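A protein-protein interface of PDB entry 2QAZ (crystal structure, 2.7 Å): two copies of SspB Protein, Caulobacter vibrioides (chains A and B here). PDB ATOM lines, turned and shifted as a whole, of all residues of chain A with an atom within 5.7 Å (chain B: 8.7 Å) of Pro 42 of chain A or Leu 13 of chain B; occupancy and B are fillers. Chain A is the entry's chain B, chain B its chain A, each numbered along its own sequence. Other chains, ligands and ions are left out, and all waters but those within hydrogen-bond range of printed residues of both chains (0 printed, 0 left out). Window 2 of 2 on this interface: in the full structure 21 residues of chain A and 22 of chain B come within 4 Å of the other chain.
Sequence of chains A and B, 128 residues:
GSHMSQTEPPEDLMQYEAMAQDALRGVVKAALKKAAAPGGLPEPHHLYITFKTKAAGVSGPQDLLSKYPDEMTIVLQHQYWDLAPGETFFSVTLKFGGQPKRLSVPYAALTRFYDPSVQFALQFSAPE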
ATOM      1  N   LYS A  34      34.673   8.340   6.104  1.00  0.00           N
ATOM      2  CA  LYS A  34      34.411   9.140   7.291  1.00  0.00           C
ATOM      3  C   LYS A  34      34.617   8.246   8.510  1.00  0.00           C
ATOM      4  O   LYS A  34      35.140   8.686   9.534  1.00  0.00           O
ATOM      5  CB  LYS A  34      32.983   9.686   7.285  1.00  0.00           C
ATOM      6  CG  LYS A  34      32.770  10.866   6.348  1.00  0.00           C
ATOM      7  CD  LYS A  34      31.320  11.342   6.353  1.00  0.00           C
ATOM      8  CE  LYS A  34      31.154  12.603   5.509  1.00  0.00           C
ATOM      9  NZ  LYS A  34      29.745  13.106   5.512  1.00  0.00           N
ATOM     10  N   GLY A  39      37.943   8.889  15.476  1.00  0.00           N
ATOM     11  CA  GLY A  39      36.728   9.526  15.954  1.00  0.00           C
ATOM     12  C   GLY A  39      35.544   8.818  15.320  1.00  0.00           C
ATOM     13  O   GLY A  39      34.403   8.930  15.774  1.00  0.00           O
ATOM     14  N   GLY A  40      35.834   8.087  14.246  1.00  0.00           N
ATOM     15  CA  GLY A  40      34.822   7.327  13.539  1.00  0.00           C
ATOM     16  C   GLY A  40      33.569   8.075  13.140  1.00  0.00           C
ATOM     17  O   GLY A  40      33.605   9.261  12.806  1.00  0.00           O
ATOM     18  N   LEU A  41      32.458   7.352  13.165  1.00  0.00           N
ATOM     19  CA  LEU A  41      31.164   7.897  12.808  1.00  0.00           C
ATOM     20  C   LEU A  41      30.563   8.623  13.998  1.00  0.00           C
ATOM     21  O   LEU A  41      30.805   8.254  15.141  1.00  0.00           O
ATOM     22  CB  LEU A  41      30.221   6.763  12.407  1.00  0.00           C
ATOM     23  CG  LEU A  41      30.646   5.854  11.257  1.00  0.00           C
ATOM     24  CD1 LEU A  41      29.805   4.587  11.254  1.00  0.00           C
ATOM     25  CD2 LEU A  41      30.502   6.607   9.954  1.00  0.00           C
ATOM     26  N   PRO A  42      29.766   9.666  13.744  1.00  0.00           N
ATOM     27  CA  PRO A  42      29.141  10.411  14.839  1.00  0.00           C
ATOM     28  C   PRO A  42      28.042   9.543  15.451  1.00  0.00           C
ATOM     29  O   PRO A  42      27.192   9.023  14.729  1.00  0.00           O
ATOM     30  CB  PRO A  42      28.550  11.634  14.140  1.00  0.00           C
ATOM     31  CG  PRO A  42      29.358  11.758  12.877  1.00  0.00           C
ATOM     32  CD  PRO A  42      29.526  10.333  12.455  1.00  0.00           C
ATOM     33  N   GLU A  43      28.060   9.374  16.770  1.00  0.00           N
ATOM     34  CA  GLU A  43      27.028   8.584  17.432  1.00  0.00           C
ATOM     35  C   GLU A  43      25.713   9.208  16.993  1.00  0.00           C
ATOM     36  O   GLU A  43      25.628  10.426  16.856  1.00  0.00           O
ATOM     37  CB  GLU A  43      27.156   8.712  18.944  1.00  0.00           C
ATOM     38  CG  GLU A  43      28.546   8.440  19.488  1.00  0.00           C
ATOM     39  CD  GLU A  43      28.932   6.978  19.409  1.00  0.00           C
ATOM     40  OE1 GLU A  43      28.125   6.127  19.855  1.00  0.00           O
ATOM     41  OE2 GLU A  43      30.045   6.682  18.914  1.00  0.00           O
ATOM     42  N   PRO A  44      24.667   8.396  16.772  1.00  0.00           N
ATOM     43  CA  PRO A  44      24.556   6.939  16.883  1.00  0.00           C
ATOM     44  C   PRO A  44      24.552   6.234  15.517  1.00  0.00           C
ATOM     45  O   PRO A  44      23.859   5.227  15.329  1.00  0.00           O
ATOM     46  CB  PRO A  44      23.224   6.776  17.579  1.00  0.00           C
ATOM     47  CG  PRO A  44      22.399   7.787  16.828  1.00  0.00           C
ATOM     48  CD  PRO A  44      23.323   9.002  16.723  1.00  0.00           C
ATOM     49  N   HIS A  45      25.316   6.767  14.568  1.00  0.00           N
ATOM     50  CA  HIS A  45      25.376   6.196  13.229  1.00  0.00           C
ATOM     51  C   HIS A  45      26.099   4.857  13.158  1.00  0.00           C
ATOM     52  O   HIS A  45      27.286   4.778  13.442  1.00  0.00           O
ATOM     53  CB  HIS A  45      26.056   7.182  12.268  1.00  0.00           C
ATOM     54  CG  HIS A  45      25.168   8.303  11.818  1.00  0.00           C
ATOM     55  ND1 HIS A  45      24.303   8.183  10.751  1.00  0.00           N
ATOM     56  CD2 HIS A  45      24.969   9.543  12.324  1.00  0.00           C
ATOM     57  CE1 HIS A  45      23.606   9.299  10.624  1.00  0.00           C
ATOM     58  NE2 HIS A  45      23.990  10.140  11.567  1.00  0.00           N
ATOM     59  N   GLU B  11      19.090  16.983  12.665  1.00  0.00           N
ATOM     60  CA  GLU B  11      19.897  16.973  11.410  1.00  0.00           C
ATOM     61  C   GLU B  11      20.785  15.739  11.276  1.00  0.00           C
ATOM     62  O   GLU B  11      21.022  15.016  12.245  1.00  0.00           O
ATOM     63  CB  GLU B  11      20.759  18.235  11.327  1.00  0.00           C
ATOM     64  CG  GLU B  11      19.968  19.488  11.001  1.00  0.00           C
ATOM     65  CD  GLU B  11      20.846  20.720  10.898  1.00  0.00           C
ATOM     66  OE1 GLU B  11      21.398  21.144  11.938  1.00  0.00           O
ATOM     67  OE2 GLU B  11      20.987  21.259   9.779  1.00  0.00           O
ATOM     68  N   ASP B  12      21.273  15.515  10.062  1.00  0.00           N
ATOM     69  CA  ASP B  12      22.123  14.373   9.760  1.00  0.00           C
ATOM     70  C   ASP B  12      23.597  14.767   9.710  1.00  0.00           C
ATOM     71  O   ASP B  12      24.052  15.418   8.772  1.00  0.00           O
ATOM     72  CB  ASP B  12      21.678  13.758   8.429  1.00  0.00           C
ATOM     73  CG  ASP B  12      22.564  12.619   7.982  1.00  0.00           C
ATOM     74  OD1 ASP B  12      22.919  11.763   8.822  1.00  0.00           O
ATOM     75  OD2 ASP B  12      22.893  12.579   6.777  1.00  0.00           O
ATOM     76  N   LEU B  13      24.336  14.368  10.740  1.00  0.00           N
ATOM     77  CA  LEU B  13      25.760  14.672  10.839  1.00  0.00           C
ATOM     78  C   LEU B  13      26.555  13.896   9.799  1.00  0.00           C
ATOM     79  O   LEU B  13      27.712  14.213   9.513  1.00  0.00           O
ATOM     80  CB  LEU B  13      26.269  14.321  12.236  1.00  0.00           C
ATOM     81  CG  LEU B  13      25.857  15.237  13.390  1.00  0.00           C
ATOM     82  CD1 LEU B  13      24.350  15.436  13.415  1.00  0.00           C
ATOM     83  CD2 LEU B  13      26.343  14.623  14.692  1.00  0.00           C
ATOM     84  N   MET B  14      25.923  12.873   9.239  1.00  0.00           N
ATOM     85  CA  MET B  14      26.559  12.038   8.232  1.00  0.00           C
ATOM     86  C   MET B  14      26.491  12.728   6.864  1.00  0.00           C
ATOM     87  O   MET B  14      27.341  12.496   6.005  1.00  0.00           O
ATOM     88  CB  MET B  14      25.847  10.686   8.183  1.00  0.00           C
ATOM     89  CG  MET B  14      26.719   9.516   7.755  1.00  0.00           C
ATOM     90  SD  MET B  14      28.130   9.253   8.837  1.00  0.00           S
ATOM     91  CE  MET B  14      29.335   8.637   7.649  1.00  0.00           C
ATOM     92  N   GLN B  15      25.477  13.583   6.692  1.00  0.00           N
ATOM     93  CA  GLN B  15      25.237  14.338   5.452  1.00  0.00           C
ATOM     94  C   GLN B  15      25.063  13.444   4.228  1.00  0.00           C
ATOM     95  O   GLN B  15      25.770  13.599   3.228  1.00  0.00           O
ATOM     96  CB  GLN B  15      26.370  15.339   5.202  1.00  0.00           C
ATOM     97  CG  GLN B  15      26.330  16.534   6.130  1.00  0.00           C
ATOM     98  CD  GLN B  15      27.652  17.273   6.194  1.00  0.00           C
ATOM     99  OE1 GLN B  15      28.162  17.762   5.187  1.00  0.00           O
ATOM    100  NE2 GLN B  15      28.217  17.357   7.393  1.00  0.00           N
ATOM    101  N   TYR B  16      24.112  12.516   4.308  1.00  0.00           N
ATOM    102  CA  TYR B  16      23.865  11.601   3.207  1.00  0.00           C
ATOM    103  C   TYR B  16      23.334  12.303   1.965  1.00  0.00           C
ATOM    104  O   TYR B  16      23.760  12.003   0.853  1.00  0.00           O
ATOM    105  CB  TYR B  16      22.906  10.490   3.642  1.00  0.00           C
ATOM    106  CG  TYR B  16      23.570   9.420   4.482  1.00  0.00           C
ATOM    107  CD1 TYR B  16      23.229   9.240   5.822  1.00  0.00           C
ATOM    108  CD2 TYR B  16      24.568   8.607   3.942  1.00  0.00           C
ATOM    109  CE1 TYR B  16      23.864   8.279   6.601  1.00  0.00           C
ATOM    110  CE2 TYR B  16      25.211   7.643   4.714  1.00  0.00           C
ATOM    111  CZ  TYR B  16      24.854   7.485   6.039  1.00  0.00           C
ATOM    112  OH  TYR B  16      25.483   6.528   6.801  1.00  0.00           O
ATOM    113  N   MET B  19      26.347  13.529   0.309  1.00  0.00           N
ATOM    114  CA  MET B  19      27.235  12.501  -0.221  1.00  0.00           C
ATOM    115  C   MET B  19      26.570  11.848  -1.432  1.00  0.00           C
ATOM    116  O   MET B  19      27.237  11.490  -2.399  1.00  0.00           O
ATOM    117  CB  MET B  19      27.535  11.443   0.842  1.00  0.00           C
ATOM    118  CG  MET B  19      28.161  11.990   2.124  1.00  0.00           C
ATOM    119  SD  MET B  19      28.620  10.670   3.285  1.00  0.00           S
ATOM    120  CE  MET B  19      30.303  10.511   2.929  1.00  0.00           C
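No position is printed for both chains.
Of the 6 pairs that touch across the chains among the printed residues, none has its exchanged pair printed and touching as well.
The side-chain amino group (NZ) of Lys 34 of chain A is in hydrogen-bond range of the backbone carbonyl oxygen (O) of Met 14 of chain B (2.5 Å).
The side-chain carboxylate of Asp 12 of chain B sits close to a ring nitrogen (NE2) of His 45 of chain A (3.4 Å).
SD of Met 19 of chain B sits at hydrogen-bond distance from NZ of Lys 34 of chain A (3.5 Å).
Hydrophobic or aromatic side chains of chain A that line the printed part of chain B: Leu 41, Pro 42 and His 45.
Along chain A the printed residues that touch a printed residue of chain B span positions 34 to 45.
Along chain B the printed residues that touch a printed residue of chain A span positions 12 to 19.
Among the printed residues, 6 pairs touch across the chains.
Among the printed residues, no Asp or Glu carboxylate lies within 4 Å of a Lys or Arg side-chain nitrogen of the other chain.
The side-chain carboxylate of Asp 12 of chain B lies within hydrogen-bond range of the backbone NH of Gln 15 of chain B (2.8 Å).
The backbone NH (N) of Met 14 of chain B lies close to the side-chain carboxylate (OD1) of Asp 12 of chain B (3.2 Å).
OD2 of Asp 12 of chain B sits at hydrogen-bond distance from N of Tyr 16 of chain B (2.8 Å).
Met 14 of chain B touches Leu 41 of chain A (CE to CD2, 3.3 Å).
Pro 42 of chain A touches Leu 13 of chain B (CB to CD2, 3.8 Å).
CE1 of His 45 of chain A touches CB of Met 14 of chain B, at 3.6 Å.
Leu 13 of chain B touches one residue of chain A.
Printed residues of chain B within 4 Å of His 45 of chain A: Asp 12 and Met 14.
Of the printed residues of chain A, Asp 12 of chain B touches His 45 (3.1 Å).
Of the printed residues of chain B, Lys 34 of chain A touches Met 14 (2.5 Å) and Met 19 (3.4 Å).
Printed residues of chain A within 4 Å of Met 19 of chain B: Lys 34.
Of the printed residues of chain B, Leu 41 of chain A touches Met 14 (3.3 Å).
The nearest residue of chain B that does not touch Pro 42 of chain A is Met 14 of chain B (4.03 Å).
The nearest printed residue of chain A that does not touch Asp 12 of chain B is Lys 34 of chain A (7.0 Å).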
